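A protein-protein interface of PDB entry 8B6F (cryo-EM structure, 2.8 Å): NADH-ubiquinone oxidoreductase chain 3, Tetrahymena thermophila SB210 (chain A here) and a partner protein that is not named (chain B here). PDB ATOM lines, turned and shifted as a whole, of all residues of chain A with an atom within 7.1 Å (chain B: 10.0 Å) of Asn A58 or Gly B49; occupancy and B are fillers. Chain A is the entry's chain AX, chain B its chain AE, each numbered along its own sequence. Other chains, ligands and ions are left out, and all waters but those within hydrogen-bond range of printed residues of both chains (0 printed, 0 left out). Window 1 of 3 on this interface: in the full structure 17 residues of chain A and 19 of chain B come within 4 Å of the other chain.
The backbone carbonyl oxygen (O) of Gln B7 sits at hydrogen-bond distance from the backbone NH (N) of Ala A120 (2.5 Å). OD1 of Asn B48 sits at hydrogen-bond distance from ND2 of Asn A58, at 3.0 Å. OE1 of Glu A121 is in salt-bridge range of NZ of Lys B10. O of Lys B24 sits close to O of Gln A56, 3.5 Å away.
The backbone NH (N) of Leu B47 is in hydrogen-bond range of the backbone carbonyl oxygen (O) of Met B26 (2.8 Å). The indole nitrogen of Trp A118 sits close to the side-chain amide oxygen of Asn A60 (3.3 Å). NZ of Lys B10 lies within hydrogen-bond range of O of Ser B20. OG of Ser A119 is in hydrogen-bond range of OXT of Glu A121 (3.1 Å). OE2 of Glu B53 is in hydrogen-bond range of ND2 of Asn B48. The side-chain amino group (NZ) of Lys B10 lies within hydrogen-bond range of the side-chain amide oxygen (OE1) of Gln B22, 3.4 Å away.
Among the printed residues, pairs that only touch across the chains: Ser A119 with Gln B7, Ile A57 with Ile B23, Ile A57 with Met B26, Asn A58 with Gly B49, Asn A58 with Ile B23, Ile A55 with Met B26, Gln A56 with Ile B23, Glu A121 with Asn B48, Ala A120 with Lys B10 and Trp A118 with Phe B422.
Gly B49 touches just one residue of chain A: Asn A58. Of chain B, only Ile B23 and Met B26 come within 4 Å of Ile A57. Of chain B, only Lys B10 and Asn B48 come within 4 Å of Glu A121. Of the printed residues of chain A, Gln B7 touches Ser A119 and Ala A120. Of the printed residues of chain B, Ala A120 touches Gln B7 and Lys B10. Ile B51 touches none of the printed residues of chain A. Val B28 touches none of the printed residues of chain A. The nearest residue of chain A that does not touch Gly B49 is Asn A60 (4.1 Å). The nearest printed residue of chain A that does not touch Met B26 is Gln A56 (4.2 Å).
Printed residues of chain A that touch a printed residue of chain B: Ile A55, Gln A56, Ile A57, Asn A58, Trp A118, Ser A119, Ala A120 and Glu A121. Hydrophobic or aromatic side chains of chain A that line the printed part of chain B: Ile A57, Trp A118 and Ala A120. Along chain A the printed residues that touch a printed residue of chain B span positions 55 to 121. Among the printed residues, Asp or Glu carboxylates within 4 Å of a Lys or Arg side-chain nitrogen of the other chain: Glu A121 with Lys B10 (3.9 Å).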
ATOM      1  N   ILE A  55       7.165 -26.638  31.110  1.00  0.00           N
ATOM      2  CA  ILE A  55       8.601 -26.898  31.092  1.00  0.00           C
ATOM      3  C   ILE A  55       8.922 -27.969  30.058  1.00  0.00           C
ATOM      4  O   ILE A  55       9.841 -28.773  30.246  1.00  0.00           O
ATOM      5  CB  ILE A  55       9.113 -27.302  32.487  1.00  0.00           C
ATOM      6  CG1 ILE A  55       8.315 -28.494  33.027  1.00  0.00           C
ATOM      7  CG2 ILE A  55       9.032 -26.113  33.433  1.00  0.00           C
ATOM      8  CD1 ILE A  55       8.766 -28.984  34.394  1.00  0.00           C
ATOM      9  N   GLN A  56       8.161 -27.989  28.966  1.00  0.00           N
ATOM     10  CA  GLN A  56       8.349 -28.999  27.932  1.00  0.00           C
ATOM     11  C   GLN A  56       9.801 -29.060  27.480  1.00  0.00           C
ATOM     12  O   GLN A  56      10.452 -28.033  27.275  1.00  0.00           O
ATOM     13  CB  GLN A  56       7.447 -28.693  26.732  1.00  0.00           C
ATOM     14  CG  GLN A  56       7.635 -29.645  25.562  1.00  0.00           C
ATOM     15  CD  GLN A  56       6.697 -29.348  24.415  1.00  0.00           C
ATOM     16  OE1 GLN A  56       5.891 -28.424  24.481  1.00  0.00           O
ATOM     17  NE2 GLN A  56       6.796 -30.136  23.352  1.00  0.00           N
ATOM     18  N   ILE A  57      10.305 -30.281  27.331  1.00  0.00           N
ATOM     19  CA  ILE A  57      11.640 -30.525  26.806  1.00  0.00           C
ATOM     20  C   ILE A  57      11.520 -31.038  25.376  1.00  0.00           C
ATOM     21  O   ILE A  57      10.443 -31.408  24.910  1.00  0.00           O
ATOM     22  CB  ILE A  57      12.437 -31.518  27.670  1.00  0.00           C
ATOM     23  CG1 ILE A  57      11.638 -32.809  27.872  1.00  0.00           C
ATOM     24  CG2 ILE A  57      12.835 -30.874  28.979  1.00  0.00           C
ATOM     25  CD1 ILE A  57      12.384 -34.040  27.448  1.00  0.00           C
ATOM     26  N   ASN A  58      12.651 -31.058  24.678  1.00  0.00           N
ATOM     27  CA  ASN A  58      12.720 -31.558  23.313  1.00  0.00           C
ATOM     28  C   ASN A  58      13.280 -32.974  23.343  1.00  0.00           C
ATOM     29  O   ASN A  58      14.410 -33.190  23.792  1.00  0.00           O
ATOM     30  CB  ASN A  58      13.587 -30.651  22.444  1.00  0.00           C
ATOM     31  CG  ASN A  58      13.492 -30.992  20.973  1.00  0.00           C
ATOM     32  OD1 ASN A  58      12.611 -31.741  20.553  1.00  0.00           O
ATOM     33  ND2 ASN A  58      14.400 -30.440  20.178  1.00  0.00           N
ATOM     34  N   PHE A  59      12.484 -33.931  22.876  1.00  0.00           N
ATOM     35  CA  PHE A  59      12.871 -35.338  22.873  1.00  0.00           C
ATOM     36  C   PHE A  59      13.406 -35.704  21.489  1.00  0.00           C
ATOM     37  O   PHE A  59      12.817 -36.478  20.737  1.00  0.00           O
ATOM     38  CB  PHE A  59      11.678 -36.203  23.270  1.00  0.00           C
ATOM     39  CG  PHE A  59      12.018 -37.637  23.583  1.00  0.00           C
ATOM     40  CD1 PHE A  59      13.330 -38.057  23.731  1.00  0.00           C
ATOM     41  CD2 PHE A  59      11.003 -38.568  23.728  1.00  0.00           C
ATOM     42  CE1 PHE A  59      13.618 -39.377  24.019  1.00  0.00           C
ATOM     43  CE2 PHE A  59      11.285 -39.886  24.017  1.00  0.00           C
ATOM     44  CZ  PHE A  59      12.594 -40.292  24.163  1.00  0.00           C
ATOM     45  N   ASN A  60      14.554 -35.116  21.162  1.00  0.00           N
ATOM     46  CA  ASN A  60      15.178 -35.294  19.857  1.00  0.00           C
ATOM     47  C   ASN A  60      16.118 -36.491  19.812  1.00  0.00           C
ATOM     48  O   ASN A  60      16.793 -36.694  18.798  1.00  0.00           O
ATOM     49  CB  ASN A  60      15.927 -34.023  19.449  1.00  0.00           C
ATOM     50  CG  ASN A  60      16.917 -33.567  20.494  1.00  0.00           C
ATOM     51  OD1 ASN A  60      17.284 -34.324  21.390  1.00  0.00           O
ATOM     52  ND2 ASN A  60      17.356 -32.318  20.386  1.00  0.00           N
ATOM     53  N   PHE A  61      16.182 -37.282  20.882  1.00  0.00           N
ATOM     54  CA  PHE A  61      16.969 -38.509  20.915  1.00  0.00           C
ATOM     55  C   PHE A  61      16.071 -39.728  21.106  1.00  0.00           C
ATOM     56  O   PHE A  61      16.490 -40.736  21.676  1.00  0.00           O
ATOM     57  CB  PHE A  61      18.026 -38.443  22.016  1.00  0.00           C
ATOM     58  CG  PHE A  61      17.459 -38.255  23.393  1.00  0.00           C
ATOM     59  CD1 PHE A  61      17.214 -36.985  23.885  1.00  0.00           C
ATOM     60  CD2 PHE A  61      17.181 -39.345  24.200  1.00  0.00           C
ATOM     61  CE1 PHE A  61      16.695 -36.805  25.151  1.00  0.00           C
ATOM     62  CE2 PHE A  61      16.663 -39.172  25.468  1.00  0.00           C
ATOM     63  CZ  PHE A  61      16.420 -37.900  25.944  1.00  0.00           C
ATOM     64  N   TRP A 118      21.899 -36.927  18.085  1.00  0.00           N
ATOM     65  CA  TRP A 118      20.929 -35.854  18.244  1.00  0.00           C
ATOM     66  C   TRP A 118      20.653 -35.180  16.906  1.00  0.00           C
ATOM     67  O   TRP A 118      21.548 -35.023  16.071  1.00  0.00           O
ATOM     68  CB  TRP A 118      21.446 -34.829  19.255  1.00  0.00           C
ATOM     69  CG  TRP A 118      21.083 -35.148  20.671  1.00  0.00           C
ATOM     70  CD1 TRP A 118      20.313 -34.393  21.505  1.00  0.00           C
ATOM     71  CD2 TRP A 118      21.467 -36.308  21.419  1.00  0.00           C
ATOM     72  NE1 TRP A 118      20.197 -35.010  22.728  1.00  0.00           N
ATOM     73  CE2 TRP A 118      20.896 -36.187  22.700  1.00  0.00           C
ATOM     74  CE3 TRP A 118      22.240 -37.437  21.129  1.00  0.00           C
ATOM     75  CZ2 TRP A 118      21.072 -37.151  23.690  1.00  0.00           C
ATOM     76  CZ3 TRP A 118      22.414 -38.394  22.113  1.00  0.00           C
ATOM     77  CH2 TRP A 118      21.831 -38.245  23.379  1.00  0.00           C
ATOM     78  N   SER A 119      19.400 -34.782  16.705  1.00  0.00           N
ATOM     79  CA  SER A 119      18.951 -34.152  15.475  1.00  0.00           C
ATOM     80  C   SER A 119      18.396 -32.767  15.779  1.00  0.00           C
ATOM     81  O   SER A 119      18.195 -32.389  16.934  1.00  0.00           O
ATOM     82  CB  SER A 119      17.894 -35.010  14.771  1.00  0.00           C
ATOM     83  OG  SER A 119      16.778 -35.240  15.613  1.00  0.00           O
ATOM     84  N   ALA A 120      18.144 -32.005  14.711  1.00  0.00           N
ATOM     85  CA  ALA A 120      17.673 -30.633  14.878  1.00  0.00           C
ATOM     86  C   ALA A 120      16.345 -30.589  15.622  1.00  0.00           C
ATOM     87  O   ALA A 120      16.146 -29.740  16.500  1.00  0.00           O
ATOM     88  CB  ALA A 120      17.541 -29.958  13.514  1.00  0.00           C
ATOM     89  N   GLU A 121      15.424 -31.486  15.286  1.00  0.00           N
ATOM     90  CA  GLU A 121      14.134 -31.543  15.961  1.00  0.00           C
ATOM     91  C   GLU A 121      13.725 -32.990  16.212  1.00  0.00           C
ATOM     92  O   GLU A 121      13.074 -33.297  17.211  1.00  0.00           O
ATOM     93  CB  GLU A 121      13.062 -30.828  15.134  1.00  0.00           C
ATOM     94  CG  GLU A 121      11.723 -30.682  15.846  1.00  0.00           C
ATOM     95  CD  GLU A 121      11.790 -29.741  17.034  1.00  0.00           C
ATOM     96  OE1 GLU A 121      12.850 -29.116  17.242  1.00  0.00           O
ATOM     97  OE2 GLU A 121      10.780 -29.625  17.759  1.00  0.00           O
ATOM     98  OXT GLU A 121      14.038 -33.884  15.427  1.00  0.00           O
ATOM     99  N   GLN B   7      19.347 -33.375   9.303  1.00  0.00           N
ATOM    100  CA  GLN B   7      19.209 -33.703  10.714  1.00  0.00           C
ATOM    101  C   GLN B   7      19.951 -32.725  11.612  1.00  0.00           C
ATOM    102  O   GLN B   7      19.689 -32.692  12.819  1.00  0.00           O
ATOM    103  CB  GLN B   7      19.722 -35.120  10.980  1.00  0.00           C
ATOM    104  CG  GLN B   7      19.075 -36.185  10.117  1.00  0.00           C
ATOM    105  CD  GLN B   7      19.605 -37.570  10.416  1.00  0.00           C
ATOM    106  OE1 GLN B   7      20.110 -37.831  11.506  1.00  0.00           O
ATOM    107  NE2 GLN B   7      19.498 -38.468   9.443  1.00  0.00           N
ATOM    108  N   LYS B  10      17.669 -26.827  11.135  1.00  0.00           N
ATOM    109  CA  LYS B  10      16.231 -26.681  10.909  1.00  0.00           C
ATOM    110  C   LYS B  10      15.927 -25.212  10.637  1.00  0.00           C
ATOM    111  O   LYS B  10      15.817 -24.414  11.581  1.00  0.00           O
ATOM    112  CB  LYS B  10      15.425 -27.187  12.102  1.00  0.00           C
ATOM    113  CG  LYS B  10      13.933 -26.918  11.983  1.00  0.00           C
ATOM    114  CD  LYS B  10      13.153 -27.542  13.124  1.00  0.00           C
ATOM    115  CE  LYS B  10      11.677 -27.192  13.023  1.00  0.00           C
ATOM    116  NZ  LYS B  10      10.883 -27.750  14.151  1.00  0.00           N
ATOM    117  N   SER B  20       9.353 -24.134  11.942  1.00  0.00           N
ATOM    118  CA  SER B  20       9.094 -23.177  13.009  1.00  0.00           C
ATOM    119  C   SER B  20       9.400 -23.844  14.340  1.00  0.00           C
ATOM    120  O   SER B  20       9.649 -25.050  14.412  1.00  0.00           O
ATOM    121  CB  SER B  20       7.647 -22.679  12.968  1.00  0.00           C
ATOM    122  OG  SER B  20       7.351 -21.866  14.090  1.00  0.00           O
ATOM    123  N   LYS B  21       9.381 -23.039  15.400  1.00  0.00           N
ATOM    124  CA  LYS B  21       9.553 -23.560  16.749  1.00  0.00           C
ATOM    125  C   LYS B  21       8.291 -24.285  17.189  1.00  0.00           C
ATOM    126  O   LYS B  21       7.352 -23.660  17.692  1.00  0.00           O
ATOM    127  CB  LYS B  21       9.883 -22.434  17.733  1.00  0.00           C
ATOM    128  CG  LYS B  21      11.177 -21.697  17.439  1.00  0.00           C
ATOM    129  CD  LYS B  21      12.382 -22.611  17.560  1.00  0.00           C
ATOM    130  CE  LYS B  21      13.674 -21.833  17.388  1.00  0.00           C
ATOM    131  NZ  LYS B  21      14.857 -22.731  17.409  1.00  0.00           N
ATOM    132  N   GLN B  22       8.255 -25.599  17.000  1.00  0.00           N
ATOM    133  CA  GLN B  22       7.110 -26.403  17.395  1.00  0.00           C
ATOM    134  C   GLN B  22       7.137 -26.778  18.870  1.00  0.00           C
ATOM    135  O   GLN B  22       6.334 -27.612  19.299  1.00  0.00           O
ATOM    136  CB  GLN B  22       7.042 -27.667  16.535  1.00  0.00           C
ATOM    137  CG  GLN B  22       6.727 -27.393  15.075  1.00  0.00           C
ATOM    138  CD  GLN B  22       6.884 -28.622  14.208  1.00  0.00           C
ATOM    139  OE1 GLN B  22       7.855 -29.364  14.337  1.00  0.00           O
ATOM    140  NE2 GLN B  22       5.921 -28.852  13.326  1.00  0.00           N
ATOM    141  N   ILE B  23       8.034 -26.177  19.651  1.00  0.00           N
ATOM    142  CA  ILE B  23       8.212 -26.511  21.054  1.00  0.00           C
ATOM    143  C   ILE B  23       8.310 -25.220  21.853  1.00  0.00           C
ATOM    144  O   ILE B  23       8.677 -24.165  21.331  1.00  0.00           O
ATOM    145  CB  ILE B  23       9.469 -27.382  21.276  1.00  0.00           C
ATOM    146  CG1 ILE B  23       9.574 -27.812  22.739  1.00  0.00           C
ATOM    147  CG2 ILE B  23      10.721 -26.624  20.847  1.00  0.00           C
ATOM    148  CD1 ILE B  23      10.668 -28.808  23.006  1.00  0.00           C
ATOM    149  N   LYS B  24       7.969 -25.312  23.136  1.00  0.00           N
ATOM    150  CA  LYS B  24       8.153 -24.206  24.067  1.00  0.00           C
ATOM    151  C   LYS B  24       9.581 -24.275  24.597  1.00  0.00           C
ATOM    152  O   LYS B  24       9.903 -25.130  25.428  1.00  0.00           O
ATOM    153  CB  LYS B  24       7.132 -24.281  25.199  1.00  0.00           C
ATOM    154  CG  LYS B  24       6.787 -22.938  25.822  1.00  0.00           C
ATOM    155  CD  LYS B  24       7.943 -22.375  26.626  1.00  0.00           C
ATOM    156  CE  LYS B  24       7.593 -21.030  27.234  1.00  0.00           C
ATOM    157  NZ  LYS B  24       7.394 -19.988  26.195  1.00  0.00           N
ATOM    158  N   THR B  25      10.435 -23.379  24.112  1.00  0.00           N
ATOM    159  CA  THR B  25      11.844 -23.419  24.466  1.00  0.00           C
ATOM    160  C   THR B  25      12.047 -23.109  25.945  1.00  0.00           C
ATOM    161  O   THR B  25      11.248 -22.413  26.574  1.00  0.00           O
ATOM    162  CB  THR B  25      12.630 -22.422  23.615  1.00  0.00           C
ATOM    163  OG1 THR B  25      12.106 -21.103  23.814  1.00  0.00           O
ATOM    164  CG2 THR B  25      12.531 -22.786  22.143  1.00  0.00           C
ATOM    165  N   MET B  26      13.134 -23.641  26.500  1.00  0.00           N
ATOM    166  CA  MET B  26      13.477 -23.410  27.899  1.00  0.00           C
ATOM    167  C   MET B  26      14.248 -22.103  28.013  1.00  0.00           C
ATOM    168  O   MET B  26      15.372 -21.992  27.515  1.00  0.00           O
ATOM    169  CB  MET B  26      14.303 -24.568  28.452  1.00  0.00           C
ATOM    170  CG  MET B  26      13.479 -25.689  29.047  1.00  0.00           C
ATOM    171  SD  MET B  26      14.504 -26.939  29.840  1.00  0.00           S
ATOM    172  CE  MET B  26      13.248 -27.970  30.585  1.00  0.00           C
ATOM    173  N   ASN B  27      13.649 -21.115  28.667  1.00  0.00           N
ATOM    174  CA  ASN B  27      14.291 -19.828  28.918  1.00  0.00           C
ATOM    175  C   ASN B  27      14.845 -19.860  30.338  1.00  0.00           C
ATOM    176  O   ASN B  27      14.127 -19.582  31.302  1.00  0.00           O
ATOM    177  CB  ASN B  27      13.304 -18.687  28.720  1.00  0.00           C
ATOM    178  CG  ASN B  27      12.779 -18.609  27.302  1.00  0.00           C
ATOM    179  OD1 ASN B  27      13.429 -19.060  26.363  1.00  0.00           O
ATOM    180  ND2 ASN B  27      11.594 -18.034  27.142  1.00  0.00           N
ATOM    181  N   VAL B  28      16.122 -20.195  30.467  1.00  0.00           N
ATOM    182  CA  VAL B  28      16.763 -20.362  31.766  1.00  0.00           C
ATOM    183  C   VAL B  28      17.582 -19.120  32.080  1.00  0.00           C
ATOM    184  O   VAL B  28      18.111 -18.450  31.186  1.00  0.00           O
ATOM    185  CB  VAL B  28      17.644 -21.631  31.809  1.00  0.00           C
ATOM    186  CG1 VAL B  28      16.812 -22.865  31.524  1.00  0.00           C
ATOM    187  CG2 VAL B  28      18.795 -21.526  30.823  1.00  0.00           C
ATOM    188  N   LEU B  45      19.177 -17.907  28.552  1.00  0.00           N
ATOM    189  CA  LEU B  45      19.519 -18.942  27.588  1.00  0.00           C
ATOM    190  C   LEU B  45      18.250 -19.588  27.054  1.00  0.00           C
ATOM    191  O   LEU B  45      17.359 -19.945  27.830  1.00  0.00           O
ATOM    192  CB  LEU B  45      20.410 -20.000  28.234  1.00  0.00           C
ATOM    193  CG  LEU B  45      21.911 -19.890  27.999  1.00  0.00           C
ATOM    194  CD1 LEU B  45      22.629 -20.894  28.871  1.00  0.00           C
ATOM    195  CD2 LEU B  45      22.251 -20.115  26.539  1.00  0.00           C
ATOM    196  N   GLN B  46      18.174 -19.735  25.736  1.00  0.00           N
ATOM    197  CA  GLN B  46      17.064 -20.417  25.079  1.00  0.00           C
ATOM    198  C   GLN B  46      17.546 -21.809  24.689  1.00  0.00           C
ATOM    199  O   GLN B  46      18.157 -21.994  23.635  1.00  0.00           O
ATOM    200  CB  GLN B  46      16.582 -19.631  23.865  1.00  0.00           C
ATOM    201  CG  GLN B  46      15.450 -20.304  23.110  1.00  0.00           C
ATOM    202  CD  GLN B  46      15.006 -19.505  21.907  1.00  0.00           C
ATOM    203  OE1 GLN B  46      14.988 -18.277  21.936  1.00  0.00           O
ATOM    204  NE2 GLN B  46      14.653 -20.201  20.833  1.00  0.00           N
ATOM    205  N   LEU B  47      17.268 -22.788  25.545  1.00  0.00           N
ATOM    206  CA  LEU B  47      17.636 -24.171  25.290  1.00  0.00           C
ATOM    207  C   LEU B  47      16.513 -24.896  24.565  1.00  0.00           C
ATOM    208  O   LEU B  47      15.331 -24.683  24.850  1.00  0.00           O
ATOM    209  CB  LEU B  47      17.960 -24.896  26.597  1.00  0.00           C
ATOM    210  CG  LEU B  47      19.414 -24.832  27.070  1.00  0.00           C
ATOM    211  CD1 LEU B  47      19.898 -23.404  27.152  1.00  0.00           C
ATOM    212  CD2 LEU B  47      19.558 -25.514  28.416  1.00  0.00           C
ATOM    213  N   ASN B  48      16.892 -25.752  23.621  1.00  0.00           N
ATOM    214  CA  ASN B  48      15.946 -26.588  22.882  1.00  0.00           C
ATOM    215  C   ASN B  48      16.583 -27.969  22.770  1.00  0.00           C
ATOM    216  O   ASN B  48      17.393 -28.212  21.873  1.00  0.00           O
ATOM    217  CB  ASN B  48      15.637 -26.001  21.512  1.00  0.00           C
ATOM    218  CG  ASN B  48      14.622 -26.819  20.743  1.00  0.00           C
ATOM    219  OD1 ASN B  48      13.925 -27.658  21.310  1.00  0.00           O
ATOM    220  ND2 ASN B  48      14.527 -26.573  19.442  1.00  0.00           N
ATOM    221  N   GLY B  49      16.208 -28.867  23.676  1.00  0.00           N
ATOM    222  CA  GLY B  49      16.889 -30.141  23.774  1.00  0.00           C
ATOM    223  C   GLY B  49      18.207 -30.056  24.501  1.00  0.00           C
ATOM    224  O   GLY B  49      19.102 -30.867  24.245  1.00  0.00           O
ATOM    225  N   GLU B  50      18.351 -29.093  25.409  1.00  0.00           N
ATOM    226  CA  GLU B  50      19.592 -28.827  26.126  1.00  0.00           C
ATOM    227  C   GLU B  50      20.689 -28.314  25.204  1.00  0.00           C
ATOM    228  O   GLU B  50      21.875 -28.416  25.530  1.00  0.00           O
ATOM    229  CB  GLU B  50      20.074 -30.070  26.883  1.00  0.00           C
ATOM    230  CG  GLU B  50      21.044 -29.751  28.010  1.00  0.00           C
ATOM    231  CD  GLU B  50      21.108 -30.845  29.057  1.00  0.00           C
ATOM    232  OE1 GLU B  50      20.606 -31.956  28.788  1.00  0.00           O
ATOM    233  OE2 GLU B  50      21.653 -30.594  30.151  1.00  0.00           O
ATOM    234  N   ILE B  51      20.314 -27.763  24.054  1.00  0.00           N
ATOM    235  CA  ILE B  51      21.244 -27.150  23.114  1.00  0.00           C
ATOM    236  C   ILE B  51      20.939 -25.659  23.077  1.00  0.00           C
ATOM    237  O   ILE B  51      19.806 -25.258  22.784  1.00  0.00           O
ATOM    238  CB  ILE B  51      21.129 -27.774  21.715  1.00  0.00           C
ATOM    239  CG1 ILE B  51      21.512 -29.253  21.772  1.00  0.00           C
ATOM    240  CG2 ILE B  51      22.012 -27.027  20.722  1.00  0.00           C
ATOM    241  CD1 ILE B  51      21.310 -29.998  20.476  1.00  0.00           C
ATOM    242  N   ALA B  52      21.944 -24.842  23.374  1.00  0.00           N
ATOM    243  CA  ALA B  52      21.756 -23.400  23.345  1.00  0.00           C
ATOM    244  C   ALA B  52      21.292 -22.961  21.963  1.00  0.00           C
ATOM    245  O   ALA B  52      21.768 -23.460  20.942  1.00  0.00           O
ATOM    246  CB  ALA B  52      23.056 -22.688  23.718  1.00  0.00           C
ATOM    247  N   GLU B  53      20.322 -22.053  21.934  1.00  0.00           N
ATOM    248  CA  GLU B  53      19.853 -21.457  20.690  1.00  0.00           C
ATOM    249  C   GLU B  53      19.997 -19.946  20.675  1.00  0.00           C
ATOM    250  O   GLU B  53      20.487 -19.385  19.689  1.00  0.00           O
ATOM    251  CB  GLU B  53      18.388 -21.842  20.442  1.00  0.00           C
ATOM    252  CG  GLU B  53      18.197 -23.305  20.098  1.00  0.00           C
ATOM    253  CD  GLU B  53      16.769 -23.627  19.725  1.00  0.00           C
ATOM    254  OE1 GLU B  53      15.863 -22.875  20.137  1.00  0.00           O
ATOM    255  OE2 GLU B  53      16.552 -24.631  19.013  1.00  0.00           O
ATOM    256  N   GLY B 420      25.369 -23.346  18.469  1.00  0.00           N
ATOM    257  CA  GLY B 420      24.930 -24.701  18.215  1.00  0.00           C
ATOM    258  C   GLY B 420      25.433 -25.743  19.184  1.00  0.00           C
ATOM    259  O   GLY B 420      25.214 -26.936  18.961  1.00  0.00           O
ATOM    260  N   HIS B 421      26.100 -25.336  20.257  1.00  0.00           N
ATOM    261  CA  HIS B 421      26.683 -26.267  21.210  1.00  0.00           C
ATOM    262  C   HIS B 421      25.706 -26.593  22.338  1.00  0.00           C
ATOM    263  O   HIS B 421      24.715 -25.897  22.561  1.00  0.00           O
ATOM    264  CB  HIS B 421      27.971 -25.686  21.791  1.00  0.00           C
ATOM    265  CG  HIS B 421      29.143 -25.780  20.868  1.00  0.00           C
ATOM    266  ND1 HIS B 421      29.694 -26.985  20.488  1.00  0.00           N
ATOM    267  CD2 HIS B 421      29.877 -24.823  20.255  1.00  0.00           C
ATOM    268  CE1 HIS B 421      30.713 -26.766  19.677  1.00  0.00           C
ATOM    269  NE2 HIS B 421      30.845 -25.461  19.519  1.00  0.00           N
ATOM    270  N   PHE B 422      26.007 -27.675  23.051  1.00  0.00           N
ATOM    271  CA  PHE B 422      25.217 -28.096  24.195  1.00  0.00           C
ATOM    272  C   PHE B 422      25.496 -27.203  25.401  1.00  0.00           C
ATOM    273  O   PHE B 422      26.360 -26.323  25.376  1.00  0.00           O
ATOM    274  CB  PHE B 422      25.519 -29.550  24.551  1.00  0.00           C
ATOM    275  CG  PHE B 422      24.936 -30.544  23.594  1.00  0.00           C
ATOM    276  CD1 PHE B 422      25.639 -30.942  22.471  1.00  0.00           C
ATOM    277  CD2 PHE B 422      23.686 -31.093  23.824  1.00  0.00           C
ATOM    278  CE1 PHE B 422      25.103 -31.861  21.591  1.00  0.00           C
ATOM    279  CE2 PHE B 422      23.146 -32.012  22.951  1.00  0.00           C
ATOM    280  CZ  PHE B 422      23.855 -32.397  21.831  1.00  0.00           C
ATOM    281  N   LEU B 423      24.742 -27.442  26.475  1.00  0.00           N
ATOM    282  CA  LEU B 423      24.984 -26.721  27.719  1.00  0.00           C
ATOM    283  C   LEU B 423      26.327 -27.107  28.325  1.00  0.00           C
ATOM    284  O   LEU B 423      27.044 -26.254  28.858  1.00  0.00           O
ATOM    285  CB  LEU B 423      23.849 -26.993  28.706  1.00  0.00           C
ATOM    286  CG  LEU B 423      23.886 -26.218  30.025  1.00  0.00           C
ATOM    287  CD1 LEU B 423      23.754 -24.722  29.783  1.00  0.00           C
ATOM    288  CD2 LEU B 423      22.792 -26.713  30.953  1.00  0.00           C
ATOM    289  N   ALA B 424      26.684 -28.392  28.257  1.00  0.00           N
ATOM    290  CA  ALA B 424      27.975 -28.833  28.770  1.00  0.00           C
ATOM    291  C   ALA B 424      29.127 -28.233  27.976  1.00  0.00           C
ATOM    292  O   ALA B 424      30.217 -28.028  28.521  1.00  0.00           O
ATOM    293  CB  ALA B 424      28.052 -30.357  28.753  1.00  0.00           C
